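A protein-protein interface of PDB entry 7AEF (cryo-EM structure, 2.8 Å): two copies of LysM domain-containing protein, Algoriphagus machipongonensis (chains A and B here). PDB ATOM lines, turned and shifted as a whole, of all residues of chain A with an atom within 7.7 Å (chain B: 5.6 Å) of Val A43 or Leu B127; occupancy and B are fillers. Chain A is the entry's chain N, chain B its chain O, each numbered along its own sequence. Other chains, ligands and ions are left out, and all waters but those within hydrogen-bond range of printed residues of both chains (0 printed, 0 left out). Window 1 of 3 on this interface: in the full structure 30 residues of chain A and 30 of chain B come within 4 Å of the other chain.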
ATOM      1  N   TYR A  41      -0.636  -2.138 -16.469  1.00  0.00           N
ATOM      2  CA  TYR A  41      -1.074  -3.287 -17.254  1.00  0.00           C
ATOM      3  C   TYR A  41      -2.558  -3.543 -17.027  1.00  0.00           C
ATOM      4  O   TYR A  41      -3.008  -3.591 -15.882  1.00  0.00           O
ATOM      5  CB  TYR A  41      -0.286  -4.542 -16.876  1.00  0.00           C
ATOM      6  CG  TYR A  41       1.209  -4.417 -17.004  1.00  0.00           C
ATOM      7  CD1 TYR A  41       1.836  -4.641 -18.217  1.00  0.00           C
ATOM      8  CD2 TYR A  41       1.995  -4.080 -15.912  1.00  0.00           C
ATOM      9  CE1 TYR A  41       3.204  -4.534 -18.346  1.00  0.00           C
ATOM     10  CE2 TYR A  41       3.364  -3.968 -16.031  1.00  0.00           C
ATOM     11  CZ  TYR A  41       3.962  -4.196 -17.251  1.00  0.00           C
ATOM     12  OH  TYR A  41       5.321  -4.094 -17.388  1.00  0.00           O
ATOM     13  N   ARG A  42      -3.306  -3.742 -18.111  1.00  0.00           N
ATOM     14  CA  ARG A  42      -4.753  -3.934 -18.043  1.00  0.00           C
ATOM     15  C   ARG A  42      -5.192  -5.055 -18.976  1.00  0.00           C
ATOM     16  O   ARG A  42      -4.782  -5.097 -20.138  1.00  0.00           O
ATOM     17  CB  ARG A  42      -5.513  -2.652 -18.416  1.00  0.00           C
ATOM     18  CG  ARG A  42      -5.299  -1.459 -17.500  1.00  0.00           C
ATOM     19  CD  ARG A  42      -5.752  -1.773 -16.098  1.00  0.00           C
ATOM     20  NE  ARG A  42      -5.586  -0.647 -15.185  1.00  0.00           N
ATOM     21  CZ  ARG A  42      -4.564  -0.499 -14.351  1.00  0.00           C
ATOM     22  NH1 ARG A  42      -3.596  -1.394 -14.313  1.00  0.00           N
ATOM     23  NH2 ARG A  42      -4.510   0.554 -13.557  1.00  0.00           N
ATOM     24  N   VAL A  43      -6.028  -5.962 -18.472  1.00  0.00           N
ATOM     25  CA  VAL A  43      -6.625  -7.038 -19.263  1.00  0.00           C
ATOM     26  C   VAL A  43      -8.137  -6.959 -19.101  1.00  0.00           C
ATOM     27  O   VAL A  43      -8.635  -6.823 -17.979  1.00  0.00           O
ATOM     28  CB  VAL A  43      -6.111  -8.438 -18.851  1.00  0.00           C
ATOM     29  CG1 VAL A  43      -6.627  -9.499 -19.804  1.00  0.00           C
ATOM     30  CG2 VAL A  43      -4.606  -8.491 -18.830  1.00  0.00           C
ATOM     31  N   GLU A  44      -8.858  -7.018 -20.220  1.00  0.00           N
ATOM     32  CA  GLU A  44     -10.312  -6.879 -20.233  1.00  0.00           C
ATOM     33  C   GLU A  44     -11.049  -8.180 -20.530  1.00  0.00           C
ATOM     34  O   GLU A  44     -10.660  -8.947 -21.414  1.00  0.00           O
ATOM     35  CB  GLU A  44     -10.734  -5.798 -21.231  1.00  0.00           C
ATOM     36  CG  GLU A  44     -12.236  -5.596 -21.336  1.00  0.00           C
ATOM     37  CD  GLU A  44     -12.616  -4.526 -22.333  1.00  0.00           C
ATOM     38  OE1 GLU A  44     -11.710  -3.990 -23.003  1.00  0.00           O
ATOM     39  OE2 GLU A  44     -13.825  -4.247 -22.480  1.00  0.00           O
ATOM     40  N   GLN A  45     -12.124  -8.419 -19.782  1.00  0.00           N
ATOM     41  CA  GLN A  45     -12.924  -9.624 -19.927  1.00  0.00           C
ATOM     42  C   GLN A  45     -14.382  -9.278 -20.186  1.00  0.00           C
ATOM     43  O   GLN A  45     -14.835  -8.167 -19.914  1.00  0.00           O
ATOM     44  CB  GLN A  45     -12.844 -10.516 -18.682  1.00  0.00           C
ATOM     45  CG  GLN A  45     -11.561 -11.293 -18.549  1.00  0.00           C
ATOM     46  CD  GLN A  45     -10.599 -10.629 -17.610  1.00  0.00           C
ATOM     47  OE1 GLN A  45     -10.970  -9.733 -16.869  1.00  0.00           O
ATOM     48  NE2 GLN A  45      -9.351 -11.057 -17.643  1.00  0.00           N
ATOM     49  N   ILE A  58     -16.158 -16.066 -16.802  1.00  0.00           N
ATOM     50  CA  ILE A  58     -15.632 -14.870 -17.436  1.00  0.00           C
ATOM     51  C   ILE A  58     -14.764 -15.186 -18.633  1.00  0.00           C
ATOM     52  O   ILE A  58     -13.927 -16.031 -18.572  1.00  0.00           O
ATOM     53  CB  ILE A  58     -14.940 -13.976 -16.401  1.00  0.00           C
ATOM     54  CG1 ILE A  58     -13.803 -14.715 -15.699  1.00  0.00           C
ATOM     55  CG2 ILE A  58     -15.962 -13.518 -15.386  1.00  0.00           C
ATOM     56  CD1 ILE A  58     -12.957 -13.836 -14.817  1.00  0.00           C
ATOM     57  N   ARG A  59     -14.956 -14.442 -19.711  1.00  0.00           N
ATOM     58  CA  ARG A  59     -14.291 -14.682 -20.979  1.00  0.00           C
ATOM     59  C   ARG A  59     -13.229 -13.682 -21.327  1.00  0.00           C
ATOM     60  O   ARG A  59     -13.364 -12.552 -20.984  1.00  0.00           O
ATOM     61  CB  ARG A  59     -15.340 -14.636 -22.080  1.00  0.00           C
ATOM     62  CG  ARG A  59     -16.636 -15.349 -21.794  1.00  0.00           C
ATOM     63  CD  ARG A  59     -17.727 -14.880 -22.717  1.00  0.00           C
ATOM     64  NE  ARG A  59     -18.974 -15.593 -22.508  1.00  0.00           N
ATOM     65  CZ  ARG A  59     -19.874 -15.317 -21.573  1.00  0.00           C
ATOM     66  NH1 ARG A  59     -19.694 -14.335 -20.730  1.00  0.00           N
ATOM     67  NH2 ARG A  59     -20.966 -16.031 -21.489  1.00  0.00           N
ATOM     68  N   PHE A  60     -12.167 -14.098 -21.998  1.00  0.00           N
ATOM     69  CA  PHE A  60     -11.105 -13.196 -22.445  1.00  0.00           C
ATOM     70  C   PHE A  60     -11.588 -12.293 -23.566  1.00  0.00           C
ATOM     71  O   PHE A  60     -12.194 -12.744 -24.493  1.00  0.00           O
ATOM     72  CB  PHE A  60      -9.904 -14.022 -22.929  1.00  0.00           C
ATOM     73  CG  PHE A  60      -8.810 -13.228 -23.592  1.00  0.00           C
ATOM     74  CD1 PHE A  60      -8.112 -12.273 -22.903  1.00  0.00           C
ATOM     75  CD2 PHE A  60      -8.469 -13.457 -24.906  1.00  0.00           C
ATOM     76  CE1 PHE A  60      -7.112 -11.564 -23.510  1.00  0.00           C
ATOM     77  CE2 PHE A  60      -7.483 -12.732 -25.525  1.00  0.00           C
ATOM     78  CZ  PHE A  60      -6.802 -11.779 -24.825  1.00  0.00           C
ATOM     79  N   ASN A  61     -11.306 -11.009 -23.459  1.00  0.00           N
ATOM     80  CA  ASN A  61     -11.630 -10.048 -24.487  1.00  0.00           C
ATOM     81  C   ASN A  61     -10.306  -9.609 -25.146  1.00  0.00           C
ATOM     82  O   ASN A  61      -9.962 -10.114 -26.180  1.00  0.00           O
ATOM     83  CB  ASN A  61     -12.440  -8.877 -23.904  1.00  0.00           C
ATOM     84  CG  ASN A  61     -12.905  -7.873 -24.939  1.00  0.00           C
ATOM     85  OD1 ASN A  61     -12.599  -7.954 -26.082  1.00  0.00           O
ATOM     86  ND2 ASN A  61     -13.634  -6.913 -24.506  1.00  0.00           N
ATOM     87  N   LYS A  62      -9.525  -8.747 -24.516  1.00  0.00           N
ATOM     88  CA  LYS A  62      -8.280  -8.250 -25.099  1.00  0.00           C
ATOM     89  C   LYS A  62      -7.315  -7.653 -24.111  1.00  0.00           C
ATOM     90  O   LYS A  62      -7.660  -7.422 -23.001  1.00  0.00           O
ATOM     91  CB  LYS A  62      -8.548  -7.238 -26.201  1.00  0.00           C
ATOM     92  CG  LYS A  62      -9.042  -5.908 -25.746  1.00  0.00           C
ATOM     93  CD  LYS A  62      -9.839  -5.331 -26.859  1.00  0.00           C
ATOM     94  CE  LYS A  62     -10.752  -4.259 -26.352  1.00  0.00           C
ATOM     95  NZ  LYS A  62     -11.753  -3.989 -27.393  1.00  0.00           N
ATOM     96  N   ILE A  63      -6.087  -7.428 -24.530  1.00  0.00           N
ATOM     97  CA  ILE A  63      -5.080  -6.833 -23.685  1.00  0.00           C
ATOM     98  C   ILE A  63      -4.862  -5.394 -24.146  1.00  0.00           C
ATOM     99  O   ILE A  63      -4.554  -5.152 -25.290  1.00  0.00           O
ATOM    100  CB  ILE A  63      -3.786  -7.656 -23.722  1.00  0.00           C
ATOM    101  CG1 ILE A  63      -4.049  -9.059 -23.224  1.00  0.00           C
ATOM    102  CG2 ILE A  63      -2.721  -7.065 -22.843  1.00  0.00           C
ATOM    103  CD1 ILE A  63      -2.972 -10.046 -23.523  1.00  0.00           C
ATOM    104  N   LEU A  64      -5.088  -4.444 -23.248  1.00  0.00           N
ATOM    105  CA  LEU A  64      -4.940  -3.011 -23.524  1.00  0.00           C
ATOM    106  C   LEU A  64      -3.501  -2.514 -23.580  1.00  0.00           C
ATOM    107  O   LEU A  64      -2.622  -3.134 -23.028  1.00  0.00           O
ATOM    108  CB  LEU A  64      -5.729  -2.202 -22.515  1.00  0.00           C
ATOM    109  CG  LEU A  64      -7.222  -2.489 -22.495  1.00  0.00           C
ATOM    110  CD1 LEU A  64      -7.883  -1.665 -21.441  1.00  0.00           C
ATOM    111  CD2 LEU A  64      -7.868  -2.216 -23.831  1.00  0.00           C
ATOM    112  N   VAL B 101       1.839 -14.769 -15.120  1.00  0.00           N
ATOM    113  CA  VAL B 101       0.521 -14.208 -14.853  1.00  0.00           C
ATOM    114  C   VAL B 101      -0.005 -13.282 -15.954  1.00  0.00           C
ATOM    115  O   VAL B 101      -1.217 -13.045 -16.013  1.00  0.00           O
ATOM    116  CB  VAL B 101       0.497 -13.492 -13.483  1.00  0.00           C
ATOM    117  CG1 VAL B 101       1.022 -14.410 -12.387  1.00  0.00           C
ATOM    118  CG2 VAL B 101       1.273 -12.180 -13.518  1.00  0.00           C
ATOM    119  N   TYR B 102       0.845 -12.779 -16.842  1.00  0.00           N
ATOM    120  CA  TYR B 102       0.411 -11.738 -17.776  1.00  0.00           C
ATOM    121  C   TYR B 102       0.474 -12.131 -19.244  1.00  0.00           C
ATOM    122  O   TYR B 102      -0.434 -11.783 -20.002  1.00  0.00           O
ATOM    123  CB  TYR B 102       1.244 -10.464 -17.552  1.00  0.00           C
ATOM    124  CG  TYR B 102       0.900  -9.331 -18.489  1.00  0.00           C
ATOM    125  CD1 TYR B 102      -0.279  -8.613 -18.341  1.00  0.00           C
ATOM    126  CD2 TYR B 102       1.760  -8.974 -19.518  1.00  0.00           C
ATOM    127  CE1 TYR B 102      -0.595  -7.582 -19.201  1.00  0.00           C
ATOM    128  CE2 TYR B 102       1.453  -7.953 -20.374  1.00  0.00           C
ATOM    129  CZ  TYR B 102       0.281  -7.262 -20.214  1.00  0.00           C
ATOM    130  OH  TYR B 102      -0.006  -6.238 -21.073  1.00  0.00           O
ATOM    131  N   PRO B 111      -4.192 -15.436 -22.204  1.00  0.00           N
ATOM    132  CA  PRO B 111      -3.328 -15.642 -21.030  1.00  0.00           C
ATOM    133  C   PRO B 111      -3.738 -16.871 -20.224  1.00  0.00           C
ATOM    134  O   PRO B 111      -4.764 -17.500 -20.476  1.00  0.00           O
ATOM    135  CB  PRO B 111      -3.514 -14.356 -20.222  1.00  0.00           C
ATOM    136  CG  PRO B 111      -4.002 -13.352 -21.195  1.00  0.00           C
ATOM    137  CD  PRO B 111      -4.820 -14.098 -22.181  1.00  0.00           C
ATOM    138  N   LEU B 114      -4.832 -19.443 -13.578  1.00  0.00           N
ATOM    139  CA  LEU B 114      -3.981 -19.303 -12.406  1.00  0.00           C
ATOM    140  C   LEU B 114      -4.592 -20.009 -11.208  1.00  0.00           C
ATOM    141  O   LEU B 114      -5.799 -19.939 -10.991  1.00  0.00           O
ATOM    142  CB  LEU B 114      -3.756 -17.833 -12.052  1.00  0.00           C
ATOM    143  CG  LEU B 114      -3.253 -16.894 -13.137  1.00  0.00           C
ATOM    144  CD1 LEU B 114      -3.287 -15.469 -12.628  1.00  0.00           C
ATOM    145  CD2 LEU B 114      -1.857 -17.285 -13.588  1.00  0.00           C
ATOM    146  N   GLY B 125      -8.493 -18.271 -11.064  1.00  0.00           N
ATOM    147  CA  GLY B 125      -9.048 -17.223 -11.890  1.00  0.00           C
ATOM    148  C   GLY B 125      -8.100 -16.601 -12.886  1.00  0.00           C
ATOM    149  O   GLY B 125      -7.251 -17.275 -13.468  1.00  0.00           O
ATOM    150  N   TYR B 126      -8.277 -15.295 -13.082  1.00  0.00           N
ATOM    151  CA  TYR B 126      -7.637 -14.501 -14.124  1.00  0.00           C
ATOM    152  C   TYR B 126      -7.083 -13.211 -13.547  1.00  0.00           C
ATOM    153  O   TYR B 126      -7.675 -12.619 -12.647  1.00  0.00           O
ATOM    154  CB  TYR B 126      -8.626 -14.107 -15.217  1.00  0.00           C
ATOM    155  CG  TYR B 126      -8.849 -15.109 -16.304  1.00  0.00           C
ATOM    156  CD1 TYR B 126      -7.856 -15.998 -16.678  1.00  0.00           C
ATOM    157  CD2 TYR B 126     -10.069 -15.170 -16.954  1.00  0.00           C
ATOM    158  CE1 TYR B 126      -8.073 -16.914 -17.681  1.00  0.00           C
ATOM    159  CE2 TYR B 126     -10.299 -16.080 -17.950  1.00  0.00           C
ATOM    160  CZ  TYR B 126      -9.302 -16.946 -18.309  1.00  0.00           C
ATOM    161  OH  TYR B 126      -9.542 -17.849 -19.306  1.00  0.00           O
ATOM    162  N   LEU B 127      -5.979 -12.745 -14.118  1.00  0.00           N
ATOM    163  CA  LEU B 127      -5.471 -11.416 -13.807  1.00  0.00           C
ATOM    164  C   LEU B 127      -6.313 -10.344 -14.496  1.00  0.00           C
ATOM    165  O   LEU B 127      -6.669 -10.471 -15.667  1.00  0.00           O
ATOM    166  CB  LEU B 127      -4.013 -11.294 -14.245  1.00  0.00           C
ATOM    167  CG  LEU B 127      -3.342  -9.920 -14.173  1.00  0.00           C
ATOM    168  CD1 LEU B 127      -2.988  -9.579 -12.753  1.00  0.00           C
ATOM    169  CD2 LEU B 127      -2.119  -9.867 -15.040  1.00  0.00           C
ATOM    170  N   LYS B 128      -6.629  -9.283 -13.763  1.00  0.00           N
ATOM    171  CA  LYS B 128      -7.281  -8.117 -14.348  1.00  0.00           C
ATOM    172  C   LYS B 128      -6.393  -6.884 -14.410  1.00  0.00           C
ATOM    173  O   LYS B 128      -6.424  -6.169 -15.406  1.00  0.00           O
ATOM    174  CB  LYS B 128      -8.549  -7.770 -13.573  1.00  0.00           C
ATOM    175  CG  LYS B 128      -9.532  -8.890 -13.459  1.00  0.00           C
ATOM    176  CD  LYS B 128     -10.542  -8.591 -12.382  1.00  0.00           C
ATOM    177  CE  LYS B 128     -11.624  -7.674 -12.899  1.00  0.00           C
ATOM    178  NZ  LYS B 128     -12.723  -7.522 -11.930  1.00  0.00           N
ATOM    179  N   GLU B 129      -5.602  -6.615 -13.372  1.00  0.00           N
ATOM    180  CA  GLU B 129      -4.897  -5.350 -13.234  1.00  0.00           C
ATOM    181  C   GLU B 129      -3.555  -5.554 -12.553  1.00  0.00           C
ATOM    182  O   GLU B 129      -3.410  -6.416 -11.689  1.00  0.00           O
ATOM    183  CB  GLU B 129      -5.704  -4.343 -12.417  1.00  0.00           C
ATOM    184  CG  GLU B 129      -6.684  -3.558 -13.223  1.00  0.00           C
ATOM    185  CD  GLU B 129      -7.736  -2.919 -12.360  1.00  0.00           C
ATOM    186  OE1 GLU B 129      -7.369  -2.307 -11.336  1.00  0.00           O
ATOM    187  OE2 GLU B 129      -8.932  -3.032 -12.697  1.00  0.00           O
ATOM    188  N   MET B 130      -2.587  -4.723 -12.929  1.00  0.00           N
ATOM    189  CA  MET B 130      -1.258  -4.777 -12.340  1.00  0.00           C
ATOM    190  C   MET B 130      -0.576  -3.420 -12.478  1.00  0.00           C
ATOM    191  O   MET B 130      -0.734  -2.739 -13.491  1.00  0.00           O
ATOM    192  CB  MET B 130      -0.418  -5.879 -12.991  1.00  0.00           C
ATOM    193  CG  MET B 130       0.763  -6.311 -12.162  1.00  0.00           C
ATOM    194  SD  MET B 130       1.493  -7.851 -12.714  1.00  0.00           S
ATOM    195  CE  MET B 130       1.866  -7.486 -14.422  1.00  0.00           C
ATOM    196  N   THR B 150      -1.926  -5.998  -7.386  1.00  0.00           N
ATOM    197  CA  THR B 150      -2.515  -7.019  -8.245  1.00  0.00           C
ATOM    198  C   THR B 150      -4.005  -7.166  -7.928  1.00  0.00           C
ATOM    199  O   THR B 150      -4.429  -6.979  -6.788  1.00  0.00           O
ATOM    200  CB  THR B 150      -1.760  -8.360  -8.062  1.00  0.00           C
ATOM    201  OG1 THR B 150      -0.352  -8.139  -8.170  1.00  0.00           O
ATOM    202  CG2 THR B 150      -2.107  -9.349  -9.130  1.00  0.00           C
ATOM    203  N   LYS B 151      -4.799  -7.492  -8.947  1.00  0.00           N
ATOM    204  CA  LYS B 151      -6.224  -7.771  -8.793  1.00  0.00           C
ATOM    205  C   LYS B 151      -6.603  -9.002  -9.606  1.00  0.00           C
ATOM    206  O   LYS B 151      -6.327  -9.058 -10.806  1.00  0.00           O
ATOM    207  CB  LYS B 151      -7.057  -6.569  -9.230  1.00  0.00           C
ATOM    208  CG  LYS B 151      -8.527  -6.705  -8.946  1.00  0.00           C
ATOM    209  CD  LYS B 151      -9.280  -5.474  -9.385  1.00  0.00           C
ATOM    210  CE  LYS B 151     -10.773  -5.698  -9.296  1.00  0.00           C
ATOM    211  NZ  LYS B 151     -11.557  -4.555  -9.818  1.00  0.00           N
ATOM    212  N   ILE B 152      -7.241  -9.982  -8.962  1.00  0.00           N
ATOM    213  CA  ILE B 152      -7.554 -11.277  -9.567  1.00  0.00           C
ATOM    214  C   ILE B 152      -9.065 -11.479  -9.584  1.00  0.00           C
ATOM    215  O   ILE B 152      -9.738 -11.259  -8.572  1.00  0.00           O
ATOM    216  CB  ILE B 152      -6.873 -12.444  -8.818  1.00  0.00           C
ATOM    217  CG1 ILE B 152      -5.411 -12.135  -8.506  1.00  0.00           C
ATOM    218  CG2 ILE B 152      -6.964 -13.733  -9.616  1.00  0.00           C
ATOM    219  CD1 ILE B 152      -4.497 -12.162  -9.703  1.00  0.00           C
ATOM    220  N   GLY B 153      -9.594 -11.923 -10.725  1.00  0.00           N
ATOM    221  CA  GLY B 153     -10.981 -12.332 -10.829  1.00  0.00           C
ATOM    222  C   GLY B 153     -11.162 -13.823 -10.603  1.00  0.00           C
ATOM    223  O   GLY B 153     -10.202 -14.563 -10.470  1.00  0.00           O
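N of Tyr A41 sits at hydrogen-bond distance from O of Met B130, 3.0 Å away. The guanidinium group of Arg A42 lies within hydrogen-bond range of the backbone carbonyl oxygen of Met B130 (3.3 Å). The backbone carbonyl oxygen of Lys B128 lies within hydrogen-bond range of the backbone NH of Val A43. The side-chain amide nitrogen (NE2) of Gln A45 sits at hydrogen-bond distance from the backbone carbonyl oxygen (O) of Leu B127, at 3.4 Å.
The backbone carbonyl oxygen of Arg A42 sits at hydrogen-bond distance from the backbone NH of Leu A64 (3.2 Å). O of Tyr B126 lies within hydrogen-bond range of N of Gly B153, at 2.8 Å. The backbone NH (N) of Lys B128 sits at hydrogen-bond distance from the backbone carbonyl oxygen (O) of Lys B151. O of Glu B129 is in hydrogen-bond range of N of Lys B151 (3.3 Å).
CD1 of Tyr A41 touches CZ of Tyr B102 (3.6 Å). Tyr A41 touches Glu B129. Lys B128 touches Arg A42. Glu B129 touches Arg A42 (CG to CD, 3.5 Å). Leu B127 touches Val A43. Gln A45 touches Tyr B126. OE1 of Gln A45 touches CG of Lys B128 (3.8 Å). Ile A58 touches Tyr B126 (O to CE2, 3.7 Å). Phe A60 touches Pro B111. CG2 of Ile A63 touches OH of Tyr B102, 3.3 Å away.
Printed residues of chain B within 4 Å of Ile A58: Tyr B126. Arg A59 touches none of the printed residues of chain B. Of the printed residues of chain A, Tyr B102 touches Tyr A41 and Ile A63. Printed residues of chain A within 4 Å of Pro B111: Phe A60 (3.7 Å). Leu B127 touches just these residues of chain A: Val A43 and Gln A45. The nearest residue of chain B that does not touch Val A43 is Tyr B102 (4.1 Å). The nearest printed residue of chain B that does not touch Gln A45 is Gly B153 (6.6 Å).
Hydrophobic or aromatic side chains of chain A that line the printed part of chain B: Tyr A41, Val A43, Ile A58, Phe A60 and Ile A63. Of the 14 printed residues of chain B, 7 touch a printed residue of chain A. Printed residues of chain B that touch a printed residue of chain A: Tyr B102, Pro B111, Tyr B126, Leu B127, Lys B128, Glu B129 and Met B130. Hydrophobic or aromatic side chains of chain B that line the printed part of chain A: Tyr B102, Pro B111, Tyr B126 and Met B130. Among the printed residues, no Asp or Glu carboxylate lies within 4 Å of a Lys or Arg side-chain nitrogen of the other chain.
No position is printed for both chains.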
